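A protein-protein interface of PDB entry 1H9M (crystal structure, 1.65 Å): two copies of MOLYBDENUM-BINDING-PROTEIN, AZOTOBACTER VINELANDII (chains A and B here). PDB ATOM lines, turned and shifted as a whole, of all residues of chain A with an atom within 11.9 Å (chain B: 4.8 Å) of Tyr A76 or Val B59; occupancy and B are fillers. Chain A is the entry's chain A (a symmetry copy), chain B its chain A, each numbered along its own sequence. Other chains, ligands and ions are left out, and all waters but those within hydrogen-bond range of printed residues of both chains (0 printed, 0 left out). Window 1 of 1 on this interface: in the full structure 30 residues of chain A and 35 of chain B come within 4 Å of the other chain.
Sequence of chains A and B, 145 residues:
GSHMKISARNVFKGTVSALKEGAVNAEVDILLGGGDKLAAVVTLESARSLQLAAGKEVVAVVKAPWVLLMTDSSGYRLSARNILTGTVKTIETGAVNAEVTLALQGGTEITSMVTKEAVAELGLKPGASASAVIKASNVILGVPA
O of Ile B140 lies within hydrogen-bond range of N of Val B61, 2.8 Å away.
N of Gly B142 is in hydrogen-bond range of O of Val B59, at 2.7 Å.
The backbone carbonyl oxygen (O) of Ser A131 is in hydrogen-bond range of the backbone NH (N) of Met A70, 2.7 Å away.
OD1 of Asp A72 sits at hydrogen-bond distance from N of Ser A74 (3.0 Å).
O of Leu A68 is in hydrogen-bond range of N of Val A133, at 2.8 Å.
No position is printed for both chains.
Of the 19 pairs that touch across the chains among the printed residues, none has its exchanged pair printed and touching as well.
Printed residues of chain A that touch a printed residue of chain B: Leu A68, Met A70, Asp A72, Ser A73, Ser A74, Tyr A76, Arg A77, Leu A78, Ser A79 and Lys A135.
Hydrophobic or aromatic side chains of chain A within 4 Å of the printed part of chain B: Leu A68, Met A70, Tyr A76 and Leu A78.
Of the 14 printed residues of chain B, 8 touch a printed residue of chain A.
Hydrophobic or aromatic side chains of chain B within 4 Å of the printed part of chain A: Met B4, Val B59, Val B61, Ile B140, Val B143 and Pro B144.
Among the printed residues, no Asp or Glu carboxylate lies within 4 Å of a Lys or Arg side-chain nitrogen of the other chain.
Printed residues of chain B within 4 Å of Leu A68: Val B61 (3.97 Å) and Ile B140 (3.8 Å).
Of the printed residues of chain B, Ser A74 touches Met B4.
Tyr A76 touches just these residues of chain B: Met B4, Val B59, Gly B142, Val B143 and Pro B144.
Printed residues of chain B within 4 Å of Lys A135: Ile B140.
No residue of chain A comes within 4 Å of Val B11.
Of chain A, only Tyr A76 comes within 4 Å of Val B59.
No residue of chain A comes within 4 Å of Ala B60.
Val B61 touches just one residue of chain A: Leu A68.
Leu B141 touches two residues of chain A.
Printed residues of chain A within 4 Å of Val B143: Tyr A76 (3.2 Å) and Arg A77 (2.8 Å).
Pro B144 touches just one residue of chain A: Tyr A76.
The nearest printed residue of chain B that does not touch Tyr A76 is Lys B13 (5.1 Å).
The nearest residue of chain A that does not touch Val B59 is Leu A78 (5.2 Å).
The nearest printed residue of chain B that does not touch Met A70 is Val B61 (8.2 Å).
The backbone NH (N) of Val B143 lies within hydrogen-bond range of the backbone carbonyl oxygen (O) of Arg A77 (2.8 Å).
N of Ser A79 is in hydrogen-bond range of O of Leu B141 (2.7 Å).
Val B61 touches Leu A68 (CG1 to CD2, 3.97 Å).
Met A70 touches Met B4 (SD to CE, 3.6 Å).
Met B4 touches Asp A72.
Met B4 touches Tyr A76 (CG to CD2, 3.8 Å).
O of Val B143 touches CA of Tyr A76, 3.2 Å away.
Tyr A76 touches Pro B144 (CE1 to N, 3.6 Å).
Leu A78 touches Met B4 (CD2 to CE, 3.7 Å).
CD2 of Leu A78 touches CA of Gly B142, at 3.9 Å.
OG of Ser A79 touches CG2 of Ile B140 (3.6 Å).
CG1 of Ile B140 touches CD of Lys A135 (3.8 Å).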
ATOM      1  N   LEU A  68     -19.574  34.515  18.110  1.00  0.00           N
ATOM      2  CA  LEU A  68     -18.829  34.536  19.379  1.00  0.00           C
ATOM      3  C   LEU A  68     -17.965  35.844  19.370  1.00  0.00           C
ATOM      4  O   LEU A  68     -17.726  36.368  18.303  1.00  0.00           O
ATOM      5  CB  LEU A  68     -17.846  33.402  19.379  1.00  0.00           C
ATOM      6  CG  LEU A  68     -18.486  32.006  19.500  1.00  0.00           C
ATOM      7  CD1 LEU A  68     -19.200  31.594  18.226  1.00  0.00           C
ATOM      8  CD2 LEU A  68     -17.316  31.034  19.713  1.00  0.00           C
ATOM      9  N   LEU A  69     -17.587  36.260  20.573  1.00  0.00           N
ATOM     10  CA  LEU A  69     -16.643  37.392  20.647  1.00  0.00           C
ATOM     11  C   LEU A  69     -15.318  36.949  21.259  1.00  0.00           C
ATOM     12  O   LEU A  69     -15.342  36.156  22.195  1.00  0.00           O
ATOM     13  CB  LEU A  69     -17.178  38.570  21.466  1.00  0.00           C
ATOM     14  CG  LEU A  69     -18.402  39.249  20.791  1.00  0.00           C
ATOM     15  CD1 LEU A  69     -18.964  40.273  21.829  1.00  0.00           C
ATOM     16  CD2 LEU A  69     -18.059  39.969  19.524  1.00  0.00           C
ATOM     17  N   MET A  70     -14.197  37.427  20.716  1.00  0.00           N
ATOM     18  CA  MET A  70     -12.942  36.982  21.337  1.00  0.00           C
ATOM     19  C   MET A  70     -12.038  38.220  21.563  1.00  0.00           C
ATOM     20  O   MET A  70     -12.050  39.041  20.662  1.00  0.00           O
ATOM     21  CB  MET A  70     -12.294  35.892  20.491  1.00  0.00           C
ATOM     22  CG  MET A  70     -10.875  35.466  20.893  1.00  0.00           C
ATOM     23  SD  MET A  70     -10.356  34.116  19.781  1.00  0.00           S
ATOM     24  CE  MET A  70     -10.247  34.922  18.265  1.00  0.00           C
ATOM     25  N   THR A  71     -11.455  38.286  22.768  1.00  0.00           N
ATOM     26  CA  THR A  71     -10.539  39.456  22.888  1.00  0.00           C
ATOM     27  C   THR A  71      -9.082  39.029  22.905  1.00  0.00           C
ATOM     28  O   THR A  71      -8.212  39.895  22.854  1.00  0.00           O
ATOM     29  CB  THR A  71     -10.825  40.312  24.131  1.00  0.00           C
ATOM     30  OG1 THR A  71     -10.804  39.475  25.278  1.00  0.00           O
ATOM     31  CG2 THR A  71     -12.180  40.991  23.993  1.00  0.00           C
ATOM     32  N   ASP A  72      -8.837  37.754  23.147  1.00  0.00           N
ATOM     33  CA  ASP A  72      -7.448  37.258  23.176  1.00  0.00           C
ATOM     34  C   ASP A  72      -7.480  35.784  22.805  1.00  0.00           C
ATOM     35  O   ASP A  72      -8.009  34.978  23.569  1.00  0.00           O
ATOM     36  CB  ASP A  72      -6.860  37.443  24.571  1.00  0.00           C
ATOM     37  CG  ASP A  72      -5.446  36.922  24.740  1.00  0.00           C
ATOM     38  OD1 ASP A  72      -4.752  36.742  23.714  1.00  0.00           O
ATOM     39  OD2 ASP A  72      -5.058  36.707  25.915  1.00  0.00           O
ATOM     40  N   SER A  73      -6.874  35.441  21.673  1.00  0.00           N
ATOM     41  CA  SER A  73      -6.817  34.043  21.247  1.00  0.00           C
ATOM     42  C   SER A  73      -5.797  33.241  22.028  1.00  0.00           C
ATOM     43  O   SER A  73      -5.881  32.014  22.119  1.00  0.00           O
ATOM     44  CB  SER A  73      -6.559  33.987  19.737  1.00  0.00           C
ATOM     45  OG  SER A  73      -5.283  34.537  19.435  1.00  0.00           O
ATOM     46  N   SER A  74      -4.816  33.927  22.632  1.00  0.00           N
ATOM     47  CA  SER A  74      -3.793  33.271  23.440  1.00  0.00           C
ATOM     48  C   SER A  74      -3.023  32.240  22.613  1.00  0.00           C
ATOM     49  O   SER A  74      -2.809  31.117  23.045  1.00  0.00           O
ATOM     50  CB  SER A  74      -4.393  32.590  24.664  1.00  0.00           C
ATOM     51  OG  SER A  74      -4.943  33.528  25.574  1.00  0.00           O
ATOM     52  N   GLY A  75      -2.757  32.572  21.360  1.00  0.00           N
ATOM     53  CA  GLY A  75      -2.061  31.717  20.441  1.00  0.00           C
ATOM     54  C   GLY A  75      -2.889  30.566  19.891  1.00  0.00           C
ATOM     55  O   GLY A  75      -2.310  29.863  19.047  1.00  0.00           O
ATOM     56  N   TYR A  76      -4.150  30.351  20.290  1.00  0.00           N
ATOM     57  CA  TYR A  76      -4.915  29.272  19.642  1.00  0.00           C
ATOM     58  C   TYR A  76      -5.349  29.637  18.232  1.00  0.00           C
ATOM     59  O   TYR A  76      -5.652  30.798  17.937  1.00  0.00           O
ATOM     60  CB  TYR A  76      -6.157  28.959  20.500  1.00  0.00           C
ATOM     61  CG  TYR A  76      -5.919  27.984  21.624  1.00  0.00           C
ATOM     62  CD1 TYR A  76      -6.289  26.655  21.513  1.00  0.00           C
ATOM     63  CD2 TYR A  76      -5.306  28.396  22.808  1.00  0.00           C
ATOM     64  CE1 TYR A  76      -6.059  25.739  22.521  1.00  0.00           C
ATOM     65  CE2 TYR A  76      -5.077  27.486  23.828  1.00  0.00           C
ATOM     66  CZ  TYR A  76      -5.454  26.169  23.682  1.00  0.00           C
ATOM     67  OH  TYR A  76      -5.225  25.288  24.709  1.00  0.00           O
ATOM     68  N   ARG A  77      -5.442  28.673  17.321  1.00  0.00           N
ATOM     69  CA  ARG A  77      -5.931  28.800  15.971  1.00  0.00           C
ATOM     70  C   ARG A  77      -7.293  28.042  15.994  1.00  0.00           C
ATOM     71  O   ARG A  77      -7.279  27.000  16.610  1.00  0.00           O
ATOM     72  CB  ARG A  77      -5.005  28.187  14.901  1.00  0.00           C
ATOM     73  CG  ARG A  77      -3.607  28.790  15.049  1.00  0.00           C
ATOM     74  CD  ARG A  77      -2.634  28.263  14.004  1.00  0.00           C
ATOM     75  NE  ARG A  77      -2.374  26.830  14.132  1.00  0.00           N
ATOM     76  CZ  ARG A  77      -2.045  26.065  13.093  1.00  0.00           C
ATOM     77  NH1 ARG A  77      -1.923  26.583  11.878  1.00  0.00           N
ATOM     78  NH2 ARG A  77      -1.825  24.768  13.261  1.00  0.00           N
ATOM     79  N   LEU A  78      -8.350  28.736  15.589  1.00  0.00           N
ATOM     80  CA  LEU A  78      -9.682  28.088  15.656  1.00  0.00           C
ATOM     81  C   LEU A  78     -10.082  27.551  14.316  1.00  0.00           C
ATOM     82  O   LEU A  78      -9.717  28.071  13.266  1.00  0.00           O
ATOM     83  CB  LEU A  78     -10.721  29.186  16.071  1.00  0.00           C
ATOM     84  CG  LEU A  78     -10.430  29.800  17.451  1.00  0.00           C
ATOM     85  CD1 LEU A  78     -11.502  30.831  17.790  1.00  0.00           C
ATOM     86  CD2 LEU A  78     -10.344  28.727  18.497  1.00  0.00           C
ATOM     87  N   SER A  79     -11.043  26.597  14.270  1.00  0.00           N
ATOM     88  CA  SER A  79     -11.600  26.089  13.013  1.00  0.00           C
ATOM     89  C   SER A  79     -12.662  27.023  12.399  1.00  0.00           C
ATOM     90  O   SER A  79     -13.063  27.019  11.212  1.00  0.00           O
ATOM     91  CB  SER A  79     -12.395  24.783  13.172  1.00  0.00           C
ATOM     92  OG  SER A  79     -13.482  24.908  14.148  1.00  0.00           O
ATOM     93  N   ALA A  80     -13.177  27.902  13.296  1.00  0.00           N
ATOM     94  CA  ALA A  80     -14.190  28.842  12.784  1.00  0.00           C
ATOM     95  C   ALA A  80     -13.556  29.728  11.717  1.00  0.00           C
ATOM     96  O   ALA A  80     -12.556  30.427  11.926  1.00  0.00           O
ATOM     97  CB  ALA A  80     -14.672  29.725  13.963  1.00  0.00           C
ATOM     98  N   ARG A  81     -14.106  29.639  10.526  1.00  0.00           N
ATOM     99  CA  ARG A  81     -13.458  30.268   9.358  1.00  0.00           C
ATOM    100  C   ARG A  81     -13.543  31.797   9.325  1.00  0.00           C
ATOM    101  O   ARG A  81     -12.852  32.420   8.487  1.00  0.00           O
ATOM    102  CB  ARG A  81     -14.102  29.741   8.100  1.00  0.00           C
ATOM    103  CG  ARG A  81     -13.899  28.222   7.816  1.00  0.00           C
ATOM    104  CD  ARG A  81     -12.409  28.060   7.425  1.00  0.00           C
ATOM    105  NE  ARG A  81     -12.163  28.584   6.084  1.00  0.00           N
ATOM    106  CZ  ARG A  81     -12.550  27.890   5.006  1.00  0.00           C
ATOM    107  NH1 ARG A  81     -13.130  26.682   5.042  1.00  0.00           N
ATOM    108  NH2 ARG A  81     -12.392  28.442   3.799  1.00  0.00           N
ATOM    109  N   ASN A  82     -14.467  32.408  10.050  1.00  0.00           N
ATOM    110  CA  ASN A  82     -14.825  33.812   9.948  1.00  0.00           C
ATOM    111  C   ASN A  82     -14.382  34.534  11.209  1.00  0.00           C
ATOM    112  O   ASN A  82     -14.839  34.256  12.323  1.00  0.00           O
ATOM    113  CB  ASN A  82     -16.340  34.006   9.750  1.00  0.00           C
ATOM    114  CG  ASN A  82     -16.748  33.238   8.498  1.00  0.00           C
ATOM    115  OD1 ASN A  82     -16.065  33.435   7.483  1.00  0.00           O
ATOM    116  ND2 ASN A  82     -17.676  32.308   8.584  1.00  0.00           N
ATOM    117  N   ILE A  83     -13.276  35.332  11.081  1.00  0.00           N
ATOM    118  CA  ILE A  83     -12.816  36.061  12.268  1.00  0.00           C
ATOM    119  C   ILE A  83     -12.711  37.537  11.826  1.00  0.00           C
ATOM    120  O   ILE A  83     -12.133  37.863  10.772  1.00  0.00           O
ATOM    121  CB  ILE A  83     -11.541  35.521  12.908  1.00  0.00           C
ATOM    122  CG1 ILE A  83     -11.681  34.047  13.347  1.00  0.00           C
ATOM    123  CG2 ILE A  83     -11.145  36.394  14.101  1.00  0.00           C
ATOM    124  CD1 ILE A  83     -10.426  33.329  13.765  1.00  0.00           C
ATOM    125  N   THR A  85     -12.251  41.481  12.931  1.00  0.00           N
ATOM    126  CA  THR A  85     -11.758  42.239  14.073  1.00  0.00           C
ATOM    127  C   THR A  85     -12.104  43.721  13.998  1.00  0.00           C
ATOM    128  O   THR A  85     -12.266  44.326  12.941  1.00  0.00           O
ATOM    129  CB  THR A  85     -10.240  42.023  14.216  1.00  0.00           C
ATOM    130  OG1 THR A  85     -10.008  40.607  14.334  1.00  0.00           O
ATOM    131  CG2 THR A  85      -9.673  42.701  15.450  1.00  0.00           C
ATOM    132  N   SER A 131     -12.801  40.559  18.449  1.00  0.00           N
ATOM    133  CA  SER A 131     -13.073  39.938  17.146  1.00  0.00           C
ATOM    134  C   SER A 131     -14.413  39.122  17.220  1.00  0.00           C
ATOM    135  O   SER A 131     -14.636  38.558  18.286  1.00  0.00           O
ATOM    136  CB  SER A 131     -12.008  38.904  16.809  1.00  0.00           C
ATOM    137  OG  SER A 131     -10.717  39.536  16.700  1.00  0.00           O
ATOM    138  N   VAL A 133     -16.371  35.976  15.924  1.00  0.00           N
ATOM    139  CA  VAL A 133     -15.992  34.647  15.397  1.00  0.00           C
ATOM    140  C   VAL A 133     -17.256  33.916  14.972  1.00  0.00           C
ATOM    141  O   VAL A 133     -18.163  33.809  15.790  1.00  0.00           O
ATOM    142  CB  VAL A 133     -15.254  33.847  16.492  1.00  0.00           C
ATOM    143  CG1 VAL A 133     -14.977  32.434  16.019  1.00  0.00           C
ATOM    144  CG2 VAL A 133     -13.946  34.536  16.877  1.00  0.00           C
ATOM    145  N   LYS A 135     -18.677  30.414  12.924  1.00  0.00           N
ATOM    146  CA  LYS A 135     -18.443  29.147  12.230  1.00  0.00           C
ATOM    147  C   LYS A 135     -19.110  29.219  10.876  1.00  0.00           C
ATOM    148  O   LYS A 135     -20.223  29.709  10.651  1.00  0.00           O
ATOM    149  CB  LYS A 135     -19.175  28.082  13.118  1.00  0.00           C
ATOM    150  CG  LYS A 135     -18.590  26.681  12.800  1.00  0.00           C
ATOM    151  CD  LYS A 135     -19.127  25.636  13.783  1.00  0.00           C
ATOM    152  CE  LYS A 135     -18.953  24.264  13.138  1.00  0.00           C
ATOM    153  NZ  LYS A 135     -17.600  23.678  13.299  1.00  0.00           N
ATOM    154  N   MET B   4      -7.745  31.162  26.694  1.00  0.00           N
ATOM    155  CA  MET B   4      -8.365  32.078  25.705  1.00  0.00           C
ATOM    156  C   MET B   4      -9.385  33.000  26.386  1.00  0.00           C
ATOM    157  O   MET B   4      -9.948  32.637  27.417  1.00  0.00           O
ATOM    158  CB  MET B   4      -9.172  31.317  24.674  1.00  0.00           C
ATOM    159  CG  MET B   4      -8.450  30.413  23.701  1.00  0.00           C
ATOM    160  SD  MET B   4      -9.733  29.768  22.552  1.00  0.00           S
ATOM    161  CE  MET B   4      -9.620  30.992  21.309  1.00  0.00           C
ATOM    162  N   VAL B  11     -15.411  25.663  27.013  1.00  0.00           N
ATOM    163  CA  VAL B  11     -14.139  25.471  26.289  1.00  0.00           C
ATOM    164  C   VAL B  11     -13.552  24.184  26.893  1.00  0.00           C
ATOM    165  O   VAL B  11     -13.163  24.237  28.058  1.00  0.00           O
ATOM    166  CB  VAL B  11     -13.162  26.650  26.414  1.00  0.00           C
ATOM    167  CG1 VAL B  11     -11.834  26.299  25.693  1.00  0.00           C
ATOM    168  CG2 VAL B  11     -13.706  27.926  25.760  1.00  0.00           C
ATOM    169  N   PHE B  12     -13.645  23.079  26.180  1.00  0.00           N
ATOM    170  CA  PHE B  12     -13.228  21.785  26.697  1.00  0.00           C
ATOM    171  C   PHE B  12     -11.877  21.377  26.109  1.00  0.00           C
ATOM    172  O   PHE B  12     -11.705  21.350  24.896  1.00  0.00           O
ATOM    173  CB  PHE B  12     -14.225  20.702  26.384  1.00  0.00           C
ATOM    174  CG  PHE B  12     -15.667  20.978  26.711  1.00  0.00           C
ATOM    175  CD1 PHE B  12     -16.559  21.316  25.721  1.00  0.00           C
ATOM    176  CD2 PHE B  12     -16.136  20.835  28.012  1.00  0.00           C
ATOM    177  CE1 PHE B  12     -17.891  21.534  26.011  1.00  0.00           C
ATOM    178  CE2 PHE B  12     -17.473  21.067  28.309  1.00  0.00           C
ATOM    179  CZ  PHE B  12     -18.349  21.405  27.308  1.00  0.00           C
ATOM    180  N   LYS B  13     -10.987  20.846  26.959  1.00  0.00           N
ATOM    181  CA  LYS B  13      -9.731  20.311  26.434  1.00  0.00           C
ATOM    182  C   LYS B  13      -9.824  18.827  26.136  1.00  0.00           C
ATOM    183  O   LYS B  13     -10.482  18.046  26.815  1.00  0.00           O
ATOM    184  CB  LYS B  13      -8.605  20.549  27.462  1.00  0.00           C
ATOM    185  CG  LYS B  13      -8.217  22.011  27.615  1.00  0.00           C
ATOM    186  CD  LYS B  13      -7.141  22.203  28.668  1.00  0.00           C
ATOM    187  CE  LYS B  13      -7.031  23.648  29.143  1.00  0.00           C
ATOM    188  NZ  LYS B  13      -6.075  23.760  30.289  1.00  0.00           N
ATOM    189  N   GLU B  57      -3.653  17.456  20.455  1.00  0.00           N
ATOM    190  CA  GLU B  57      -4.470  18.044  21.567  1.00  0.00           C
ATOM    191  C   GLU B  57      -5.179  19.281  20.954  1.00  0.00           C
ATOM    192  O   GLU B  57      -4.668  20.145  20.179  1.00  0.00           O
ATOM    193  CB  GLU B  57      -3.788  18.099  22.890  1.00  0.00           C
ATOM    194  CG  GLU B  57      -2.532  17.236  23.065  1.00  0.00           C
ATOM    195  CD  GLU B  57      -1.522  17.957  23.939  1.00  0.00           C
ATOM    196  OE1 GLU B  57      -1.224  19.120  23.603  1.00  0.00           O
ATOM    197  OE2 GLU B  57      -1.064  17.374  24.938  1.00  0.00           O
ATOM    198  N   VAL B  58      -6.459  19.338  21.382  1.00  0.00           N
ATOM    199  CA  VAL B  58      -7.331  20.413  20.893  1.00  0.00           C
ATOM    200  C   VAL B  58      -8.249  20.896  22.005  1.00  0.00           C
ATOM    201  O   VAL B  58      -8.312  20.371  23.127  1.00  0.00           O
ATOM    202  CB  VAL B  58      -8.300  19.894  19.800  1.00  0.00           C
ATOM    203  CG1 VAL B  58      -7.448  19.455  18.569  1.00  0.00           C
ATOM    204  CG2 VAL B  58      -9.091  18.711  20.317  1.00  0.00           C
ATOM    205  N   VAL B  59      -8.923  22.032  21.789  1.00  0.00           N
ATOM    206  CA  VAL B  59     -10.028  22.508  22.596  1.00  0.00           C
ATOM    207  C   VAL B  59     -11.327  22.500  21.719  1.00  0.00           C
ATOM    208  O   VAL B  59     -11.210  22.598  20.501  1.00  0.00           O
ATOM    209  CB  VAL B  59      -9.832  23.948  23.129  1.00  0.00           C
ATOM    210  CG1 VAL B  59      -8.818  23.734  24.286  1.00  0.00           C
ATOM    211  CG2 VAL B  59      -9.567  24.951  22.029  1.00  0.00           C
ATOM    212  N   ALA B  60     -12.427  22.185  22.390  1.00  0.00           N
ATOM    213  CA  ALA B  60     -13.741  22.206  21.695  1.00  0.00           C
ATOM    214  C   ALA B  60     -14.454  23.421  22.315  1.00  0.00           C
ATOM    215  O   ALA B  60     -14.509  23.532  23.538  1.00  0.00           O
ATOM    216  CB  ALA B  60     -14.469  20.948  22.109  1.00  0.00           C
ATOM    217  N   VAL B  61     -15.032  24.297  21.531  1.00  0.00           N
ATOM    218  CA  VAL B  61     -15.635  25.545  21.966  1.00  0.00           C
ATOM    219  C   VAL B  61     -17.134  25.534  21.593  1.00  0.00           C
ATOM    220  O   VAL B  61     -17.400  25.350  20.405  1.00  0.00           O
ATOM    221  CB  VAL B  61     -14.944  26.703  21.212  1.00  0.00           C
ATOM    222  CG1 VAL B  61     -15.532  28.039  21.611  1.00  0.00           C
ATOM    223  CG2 VAL B  61     -13.439  26.593  21.591  1.00  0.00           C
ATOM    224  N   ILE B 140     -16.896  24.275  17.667  1.00  0.00           N
ATOM    225  CA  ILE B 140     -15.697  24.864  17.034  1.00  0.00           C
ATOM    226  C   ILE B 140     -14.497  24.179  17.677  1.00  0.00           C
ATOM    227  O   ILE B 140     -14.479  23.824  18.847  1.00  0.00           O
ATOM    228  CB  ILE B 140     -15.720  26.364  17.319  1.00  0.00           C
ATOM    229  CG1 ILE B 140     -16.777  27.033  16.430  1.00  0.00           C
ATOM    230  CG2 ILE B 140     -14.311  26.942  17.045  1.00  0.00           C
ATOM    231  CD1 ILE B 140     -17.089  28.478  16.947  1.00  0.00           C
ATOM    232  N   LEU B 141     -13.442  23.910  16.826  1.00  0.00           N
ATOM    233  CA  LEU B 141     -12.274  23.305  17.483  1.00  0.00           C
ATOM    234  C   LEU B 141     -11.146  24.327  17.447  1.00  0.00           C
ATOM    235  O   LEU B 141     -11.051  25.237  16.635  1.00  0.00           O
ATOM    236  CB  LEU B 141     -11.765  22.147  16.594  1.00  0.00           C
ATOM    237  CG  LEU B 141     -12.789  20.997  16.589  1.00  0.00           C
ATOM    238  CD1 LEU B 141     -12.202  19.840  15.682  1.00  0.00           C
ATOM    239  CD2 LEU B 141     -13.178  20.507  17.952  1.00  0.00           C
ATOM    240  N   GLY B 142     -10.258  24.136  18.467  1.00  0.00           N
ATOM    241  CA  GLY B 142      -9.089  25.037  18.511  1.00  0.00           C
ATOM    242  C   GLY B 142      -7.794  24.243  18.801  1.00  0.00           C
ATOM    243  O   GLY B 142      -7.878  23.163  19.347  1.00  0.00           O
ATOM    244  N   VAL B 143      -6.716  24.724  18.213  1.00  0.00           N
ATOM    245  CA  VAL B 143      -5.407  24.084  18.449  1.00  0.00           C
ATOM    246  C   VAL B 143      -4.477  25.169  19.015  1.00  0.00           C
ATOM    247  O   VAL B 143      -4.347  26.283  18.658  1.00  0.00           O
ATOM    248  CB  VAL B 143      -4.727  23.361  17.295  1.00  0.00           C
ATOM    249  CG1 VAL B 143      -5.533  22.130  16.886  1.00  0.00           C
ATOM    250  CG2 VAL B 143      -4.415  24.262  16.116  1.00  0.00           C
ATOM    251  N   PRO B 144      -3.715  24.540  20.031  1.00  0.00           N
ATOM    252  CA  PRO B 144      -2.762  25.411  20.745  1.00  0.00           C
ATOM    253  C   PRO B 144      -1.513  25.795  19.990  1.00  0.00           C
ATOM    254  O   PRO B 144      -1.389  25.618  18.776  1.00  0.00           O
ATOM    255  CB  PRO B 144      -2.289  24.637  21.976  1.00  0.00           C
ATOM    256  CG  PRO B 144      -3.187  23.457  22.071  1.00  0.00           C
ATOM    257  CD  PRO B 144      -3.575  23.128  20.673  1.00  0.00           C
